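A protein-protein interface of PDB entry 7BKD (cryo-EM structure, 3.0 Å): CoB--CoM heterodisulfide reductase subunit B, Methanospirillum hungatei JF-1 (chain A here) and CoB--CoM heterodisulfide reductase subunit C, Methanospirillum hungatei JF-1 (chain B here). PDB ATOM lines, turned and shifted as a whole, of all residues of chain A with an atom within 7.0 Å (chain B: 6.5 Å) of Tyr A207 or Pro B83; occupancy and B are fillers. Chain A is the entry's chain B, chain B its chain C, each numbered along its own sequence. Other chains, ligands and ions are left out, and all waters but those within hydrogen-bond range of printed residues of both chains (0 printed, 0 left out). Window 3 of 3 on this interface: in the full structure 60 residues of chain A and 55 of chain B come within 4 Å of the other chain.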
ATOM      1  N   GLY A 202       8.494  29.655  -0.840  1.00  0.00           N
ATOM      2  CA  GLY A 202       9.761  29.329  -1.465  1.00  0.00           C
ATOM      3  C   GLY A 202      10.294  27.950  -1.145  1.00  0.00           C
ATOM      4  O   GLY A 202      11.456  27.649  -1.432  1.00  0.00           O
ATOM      5  N   GLY A 203       9.459  27.099  -0.559  1.00  0.00           N
ATOM      6  CA  GLY A 203       9.912  25.815  -0.080  1.00  0.00           C
ATOM      7  C   GLY A 203      10.626  25.852   1.250  1.00  0.00           C
ATOM      8  O   GLY A 203      11.061  24.798   1.728  1.00  0.00           O
ATOM      9  N   VAL A 204      10.749  27.028   1.869  1.00  0.00           N
ATOM     10  CA  VAL A 204      11.475  27.139   3.130  1.00  0.00           C
ATOM     11  C   VAL A 204      10.819  26.273   4.196  1.00  0.00           C
ATOM     12  O   VAL A 204      11.500  25.600   4.980  1.00  0.00           O
ATOM     13  CB  VAL A 204      11.558  28.615   3.563  1.00  0.00           C
ATOM     14  CG1 VAL A 204      11.994  28.732   5.013  1.00  0.00           C
ATOM     15  CG2 VAL A 204      12.495  29.380   2.649  1.00  0.00           C
ATOM     16  N   ARG A 205       9.486  26.237   4.202  1.00  0.00           N
ATOM     17  CA  ARG A 205       8.729  25.446   5.164  1.00  0.00           C
ATOM     18  C   ARG A 205       9.084  23.971   5.079  1.00  0.00           C
ATOM     19  O   ARG A 205       8.870  23.232   6.044  1.00  0.00           O
ATOM     20  CB  ARG A 205       7.239  25.687   4.907  1.00  0.00           C
ATOM     21  CG  ARG A 205       6.204  25.094   5.856  1.00  0.00           C
ATOM     22  CD  ARG A 205       5.675  23.743   5.424  1.00  0.00           C
ATOM     23  NE  ARG A 205       4.638  23.259   6.335  1.00  0.00           N
ATOM     24  CZ  ARG A 205       4.859  22.597   7.464  1.00  0.00           C
ATOM     25  NH1 ARG A 205       6.095  22.322   7.849  1.00  0.00           N
ATOM     26  NH2 ARG A 205       3.837  22.203   8.208  1.00  0.00           N
ATOM     27  N   GLY A 206       9.638  23.530   3.953  1.00  0.00           N
ATOM     28  CA  GLY A 206      10.161  22.187   3.853  1.00  0.00           C
ATOM     29  C   GLY A 206      11.656  22.105   4.080  1.00  0.00           C
ATOM     30  O   GLY A 206      12.147  21.123   4.638  1.00  0.00           O
ATOM     31  N   TYR A 207      12.391  23.136   3.658  1.00  0.00           N
ATOM     32  CA  TYR A 207      13.847  23.043   3.617  1.00  0.00           C
ATOM     33  C   TYR A 207      14.458  23.105   5.010  1.00  0.00           C
ATOM     34  O   TYR A 207      15.099  22.152   5.461  1.00  0.00           O
ATOM     35  CB  TYR A 207      14.423  24.151   2.736  1.00  0.00           C
ATOM     36  CG  TYR A 207      15.897  24.382   2.962  1.00  0.00           C
ATOM     37  CD1 TYR A 207      16.357  25.580   3.491  1.00  0.00           C
ATOM     38  CD2 TYR A 207      16.826  23.395   2.676  1.00  0.00           C
ATOM     39  CE1 TYR A 207      17.702  25.794   3.709  1.00  0.00           C
ATOM     40  CE2 TYR A 207      18.172  23.600   2.892  1.00  0.00           C
ATOM     41  CZ  TYR A 207      18.604  24.800   3.409  1.00  0.00           C
ATOM     42  OH  TYR A 207      19.948  24.999   3.622  1.00  0.00           O
ATOM     43  N   ASP A 208      14.279  24.224   5.700  1.00  0.00           N
ATOM     44  CA  ASP A 208      14.791  24.398   7.054  1.00  0.00           C
ATOM     45  C   ASP A 208      13.607  24.854   7.896  1.00  0.00           C
ATOM     46  O   ASP A 208      13.232  26.029   7.883  1.00  0.00           O
ATOM     47  CB  ASP A 208      15.955  25.382   7.093  1.00  0.00           C
ATOM     48  CG  ASP A 208      16.416  25.685   8.496  1.00  0.00           C
ATOM     49  OD1 ASP A 208      16.276  26.837   8.926  1.00  0.00           O
ATOM     50  OD2 ASP A 208      16.923  24.764   9.173  1.00  0.00           O
ATOM     51  N   ILE A 209      12.828  23.923   8.460  1.00  0.00           N
ATOM     52  CA  ILE A 209      11.523  24.243   9.130  1.00  0.00           C
ATOM     53  C   ILE A 209      11.642  25.195  10.317  1.00  0.00           C
ATOM     54  O   ILE A 209      10.715  25.996  10.517  1.00  0.00           O
ATOM     55  CB  ILE A 209      10.788  22.923   9.496  1.00  0.00           C
ATOM     56  CG1 ILE A 209       9.519  23.140  10.325  1.00  0.00           C
ATOM     57  CG2 ILE A 209      11.736  21.952  10.180  1.00  0.00           C
ATOM     58  CD1 ILE A 209       8.367  23.719   9.544  1.00  0.00           C
ATOM     59  N   VAL A 210      12.737  25.136  11.067  1.00  0.00           N
ATOM     60  CA  VAL A 210      12.939  25.988  12.273  1.00  0.00           C
ATOM     61  C   VAL A 210      12.984  27.464  11.862  1.00  0.00           C
ATOM     62  O   VAL A 210      12.393  28.275  12.569  1.00  0.00           O
ATOM     63  CB  VAL A 210      14.220  25.531  13.007  1.00  0.00           C
ATOM     64  CG1 VAL A 210      14.690  26.553  14.029  1.00  0.00           C
ATOM     65  CG2 VAL A 210      14.025  24.173  13.654  1.00  0.00           C
ATOM     66  N   HIS A 211      13.653  27.781  10.748  1.00  0.00           N
ATOM     67  CA  HIS A 211      13.738  29.175  10.234  1.00  0.00           C
ATOM     68  C   HIS A 211      12.341  29.675   9.884  1.00  0.00           C
ATOM     69  O   HIS A 211      12.001  30.779  10.317  1.00  0.00           O
ATOM     70  CB  HIS A 211      14.623  29.160   8.981  1.00  0.00           C
ATOM     71  CG  HIS A 211      14.839  30.465   8.302  1.00  0.00           C
ATOM     72  ND1 HIS A 211      15.989  31.197   8.476  1.00  0.00           N
ATOM     73  CD2 HIS A 211      14.090  31.135   7.404  1.00  0.00           C
ATOM     74  CE1 HIS A 211      15.927  32.283   7.740  1.00  0.00           C
ATOM     75  NE2 HIS A 211      14.772  32.267   7.081  1.00  0.00           N
ATOM     76  N   PHE B  67      24.166  37.934  -2.799  1.00  0.00           N
ATOM     77  CA  PHE B  67      23.872  37.115  -3.970  1.00  0.00           C
ATOM     78  C   PHE B  67      23.825  37.958  -5.237  1.00  0.00           C
ATOM     79  O   PHE B  67      24.304  37.530  -6.294  1.00  0.00           O
ATOM     80  CB  PHE B  67      22.561  36.358  -3.769  1.00  0.00           C
ATOM     81  CG  PHE B  67      22.726  35.067  -3.035  1.00  0.00           C
ATOM     82  CD1 PHE B  67      23.296  33.970  -3.660  1.00  0.00           C
ATOM     83  CD2 PHE B  67      22.330  34.949  -1.719  1.00  0.00           C
ATOM     84  CE1 PHE B  67      23.457  32.781  -2.986  1.00  0.00           C
ATOM     85  CE2 PHE B  67      22.489  33.765  -1.041  1.00  0.00           C
ATOM     86  CZ  PHE B  67      23.052  32.676  -1.674  1.00  0.00           C
ATOM     87  N   ALA B  79      27.935  31.226  -5.132  1.00  0.00           N
ATOM     88  CA  ALA B  79      26.498  31.405  -4.964  1.00  0.00           C
ATOM     89  C   ALA B  79      25.757  30.072  -4.980  1.00  0.00           C
ATOM     90  O   ALA B  79      24.902  29.827  -4.123  1.00  0.00           O
ATOM     91  CB  ALA B  79      25.952  32.329  -6.053  1.00  0.00           C
ATOM     92  N   LEU B  80      26.075  29.198  -5.941  1.00  0.00           N
ATOM     93  CA  LEU B  80      25.339  27.944  -6.081  1.00  0.00           C
ATOM     94  C   LEU B  80      25.566  27.027  -4.888  1.00  0.00           C
ATOM     95  O   LEU B  80      24.615  26.438  -4.361  1.00  0.00           O
ATOM     96  CB  LEU B  80      25.740  27.240  -7.376  1.00  0.00           C
ATOM     97  CG  LEU B  80      25.351  27.930  -8.686  1.00  0.00           C
ATOM     98  CD1 LEU B  80      25.384  26.939  -9.830  1.00  0.00           C
ATOM     99  CD2 LEU B  80      23.983  28.583  -8.574  1.00  0.00           C
ATOM    100  N   THR B  81      26.811  26.897  -4.445  1.00  0.00           N
ATOM    101  CA  THR B  81      27.142  26.043  -3.308  1.00  0.00           C
ATOM    102  C   THR B  81      27.094  26.822  -2.002  1.00  0.00           C
ATOM    103  O   THR B  81      28.029  26.803  -1.206  1.00  0.00           O
ATOM    104  CB  THR B  81      28.512  25.413  -3.513  1.00  0.00           C
ATOM    105  OG1 THR B  81      29.526  26.388  -3.243  1.00  0.00           O
ATOM    106  CG2 THR B  81      28.655  24.930  -4.942  1.00  0.00           C
ATOM    107  N   ASP B  82      25.986  27.521  -1.776  1.00  0.00           N
ATOM    108  CA  ASP B  82      25.783  28.283  -0.553  1.00  0.00           C
ATOM    109  C   ASP B  82      24.488  27.797   0.079  1.00  0.00           C
ATOM    110  O   ASP B  82      23.415  27.931  -0.539  1.00  0.00           O
ATOM    111  CB  ASP B  82      25.729  29.784  -0.842  1.00  0.00           C
ATOM    112  CG  ASP B  82      25.631  30.618   0.417  1.00  0.00           C
ATOM    113  OD1 ASP B  82      26.679  31.092   0.897  1.00  0.00           O
ATOM    114  OD2 ASP B  82      24.515  30.805   0.934  1.00  0.00           O
ATOM    115  N   PRO B  83      24.528  27.215   1.278  1.00  0.00           N
ATOM    116  CA  PRO B  83      23.290  26.696   1.880  1.00  0.00           C
ATOM    117  C   PRO B  83      22.246  27.767   2.129  1.00  0.00           C
ATOM    118  O   PRO B  83      21.055  27.442   2.201  1.00  0.00           O
ATOM    119  CB  PRO B  83      23.758  26.052   3.194  1.00  0.00           C
ATOM    120  CG  PRO B  83      25.187  26.364   3.342  1.00  0.00           C
ATOM    121  CD  PRO B  83      25.724  26.971   2.100  1.00  0.00           C
ATOM    122  N   ASP B  84      22.641  29.030   2.259  1.00  0.00           N
ATOM    123  CA  ASP B  84      21.658  30.106   2.372  1.00  0.00           C
ATOM    124  C   ASP B  84      21.198  30.572   0.996  1.00  0.00           C
ATOM    125  O   ASP B  84      21.099  31.760   0.721  1.00  0.00           O
ATOM    126  CB  ASP B  84      22.235  31.268   3.171  1.00  0.00           C
ATOM    127  CG  ASP B  84      22.842  30.834   4.485  1.00  0.00           C
ATOM    128  OD1 ASP B  84      22.120  30.245   5.314  1.00  0.00           O
ATOM    129  OD2 ASP B  84      24.044  31.097   4.700  1.00  0.00           O
ATOM    130  N   LEU B  85      20.886  29.618   0.127  1.00  0.00           N
ATOM    131  CA  LEU B  85      20.215  29.888  -1.131  1.00  0.00           C
ATOM    132  C   LEU B  85      18.778  29.408  -1.111  1.00  0.00           C
ATOM    133  O   LEU B  85      17.971  29.861  -1.927  1.00  0.00           O
ATOM    134  CB  LEU B  85      20.968  29.221  -2.293  1.00  0.00           C
ATOM    135  CG  LEU B  85      20.406  29.266  -3.717  1.00  0.00           C
ATOM    136  CD1 LEU B  85      20.394  30.687  -4.260  1.00  0.00           C
ATOM    137  CD2 LEU B  85      21.195  28.350  -4.631  1.00  0.00           C
ATOM    138  N   TRP B  86      18.439  28.538  -0.167  1.00  0.00           N
ATOM    139  CA  TRP B  86      17.110  27.981  -0.020  1.00  0.00           C
ATOM    140  C   TRP B  86      16.373  28.556   1.179  1.00  0.00           C
ATOM    141  O   TRP B  86      15.354  27.999   1.594  1.00  0.00           O
ATOM    142  CB  TRP B  86      17.211  26.460   0.071  1.00  0.00           C
ATOM    143  CG  TRP B  86      18.183  25.921  -0.927  1.00  0.00           C
ATOM    144  CD1 TRP B  86      19.518  25.724  -0.748  1.00  0.00           C
ATOM    145  CD2 TRP B  86      17.899  25.541  -2.277  1.00  0.00           C
ATOM    146  NE1 TRP B  86      20.082  25.236  -1.897  1.00  0.00           N
ATOM    147  CE2 TRP B  86      19.108  25.113  -2.852  1.00  0.00           C
ATOM    148  CE3 TRP B  86      16.737  25.512  -3.051  1.00  0.00           C
ATOM    149  CZ2 TRP B  86      19.189  24.662  -4.161  1.00  0.00           C
ATOM    150  CZ3 TRP B  86      16.821  25.066  -4.348  1.00  0.00           C
ATOM    151  CH2 TRP B  86      18.036  24.646  -4.892  1.00  0.00           C
ATOM    152  N   LEU B  87      16.866  29.655   1.742  1.00  0.00           N
ATOM    153  CA  LEU B  87      16.174  30.355   2.812  1.00  0.00           C
ATOM    154  C   LEU B  87      15.286  31.480   2.303  1.00  0.00           C
ATOM    155  O   LEU B  87      14.572  32.093   3.102  1.00  0.00           O
ATOM    156  CB  LEU B  87      17.181  30.912   3.820  1.00  0.00           C
ATOM    157  CG  LEU B  87      17.896  29.891   4.704  1.00  0.00           C
ATOM    158  CD1 LEU B  87      18.930  30.586   5.561  1.00  0.00           C
ATOM    159  CD2 LEU B  87      16.901  29.139   5.564  1.00  0.00           C
ATOM    160  N   PRO B 122      17.754  20.678  -2.028  1.00  0.00           N
ATOM    161  CA  PRO B 122      17.144  20.019  -0.867  1.00  0.00           C
ATOM    162  C   PRO B 122      16.181  18.918  -1.291  1.00  0.00           C
ATOM    163  O   PRO B 122      15.537  18.993  -2.339  1.00  0.00           O
ATOM    164  CB  PRO B 122      16.411  21.159  -0.155  1.00  0.00           C
ATOM    165  CG  PRO B 122      17.105  22.398  -0.616  1.00  0.00           C
ATOM    166  CD  PRO B 122      17.534  22.132  -2.020  1.00  0.00           C
ATOM    167  N   LYS B 123      16.076  17.894  -0.443  1.00  0.00           N
ATOM    168  CA  LYS B 123      15.348  16.677  -0.783  1.00  0.00           C
ATOM    169  C   LYS B 123      13.835  16.855  -0.795  1.00  0.00           C
ATOM    170  O   LYS B 123      13.137  16.044  -1.415  1.00  0.00           O
ATOM    171  CB  LYS B 123      15.728  15.567   0.196  1.00  0.00           C
ATOM    172  CG  LYS B 123      17.198  15.201   0.148  1.00  0.00           C
ATOM    173  CD  LYS B 123      17.554  14.492  -1.148  1.00  0.00           C
ATOM    174  CE  LYS B 123      19.041  14.182  -1.213  1.00  0.00           C
ATOM    175  NZ  LYS B 123      19.421  13.516  -2.490  1.00  0.00           N
ATOM    176  N   ASN B 124      13.311  17.887  -0.134  1.00  0.00           N
ATOM    177  CA  ASN B 124      11.874  18.136  -0.173  1.00  0.00           C
ATOM    178  C   ASN B 124      11.399  18.433  -1.591  1.00  0.00           C
ATOM    179  O   ASN B 124      10.304  18.017  -1.984  1.00  0.00           O
ATOM    180  CB  ASN B 124      11.512  19.283   0.767  1.00  0.00           C
ATOM    181  CG  ASN B 124      12.173  20.592   0.375  1.00  0.00           C
ATOM    182  OD1 ASN B 124      12.829  20.684  -0.653  1.00  0.00           O
ATOM    183  ND2 ASN B 124      11.965  21.617   1.172  1.00  0.00           N
ATOM    184  N   PHE B 125      12.197  19.174  -2.361  1.00  0.00           N
ATOM    185  CA  PHE B 125      11.830  19.456  -3.743  1.00  0.00           C
ATOM    186  C   PHE B 125      11.722  18.170  -4.550  1.00  0.00           C
ATOM    187  O   PHE B 125      10.779  17.992  -5.330  1.00  0.00           O
ATOM    188  CB  PHE B 125      12.848  20.408  -4.374  1.00  0.00           C
ATOM    189  CG  PHE B 125      12.922  21.749  -3.705  1.00  0.00           C
ATOM    190  CD1 PHE B 125      11.912  22.677  -3.872  1.00  0.00           C
ATOM    191  CD2 PHE B 125      14.011  22.090  -2.925  1.00  0.00           C
ATOM    192  CE1 PHE B 125      11.979  23.914  -3.262  1.00  0.00           C
ATOM    193  CE2 PHE B 125      14.079  23.322  -2.309  1.00  0.00           C
ATOM    194  CZ  PHE B 125      13.064  24.235  -2.480  1.00  0.00           C
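Among the printed residues, merely in contact across the chains: Gly A206 with Asn B124, Tyr A207 with Trp B86, Val A204 with Trp B86, Val A204 with Leu B87, Tyr A207 with Pro B122, His A211 with Leu B87, Tyr A207 with Leu B87 and Gly A202 with Phe B125.
OH of Tyr A207 sits at hydrogen-bond distance from O of Pro B83 (3.0 Å).
ND2 of Asn B124 sits at hydrogen-bond distance from O of Gly A203 (3.4 Å).
N of Tyr A207 sits close to ND2 of Asn B124.
The backbone NH of His A211 sits close to the side-chain carboxylate of Asp A208 (3.3 Å).
Tyr A207 touches just these residues of chain B: Pro B83 (3.0 Å), Trp B86 (3.2 Å), Leu B87 (3.9 Å), Pro B122 (3.5 Å) and Asn B124 (2.9 Å).
Of the printed residues of chain A, Pro B83 touches Tyr A207 (3.0 Å).
Printed residues of chain B within 4 Å of Val A204: Trp B86 and Leu B87.
Of the printed residues of chain A, Trp B86 touches Val A204 and Tyr A207.
Printed residues of chain A within 4 Å of Phe B125: Gly A202.
Printed residues of chain B within 4 Å of His A211: Leu B87.
Printed residues of chain B within 4 Å of Gly A202: Phe B125.
The nearest printed residue of chain A that does not touch Pro B122 is Gly A206 (6.4 Å).
Hydrophobic or aromatic side chains of chain A that line the printed part of chain B: Val A204, Tyr A207 and His A211.
Of the 14 printed residues of chain B, 6 touch a printed residue of chain A.
Among the printed residues, 11 pairs touch across the chains.
Among the printed residues, no Asp or Glu carboxylate lies within 4 Å of a Lys or Arg side-chain nitrogen of the other chain.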
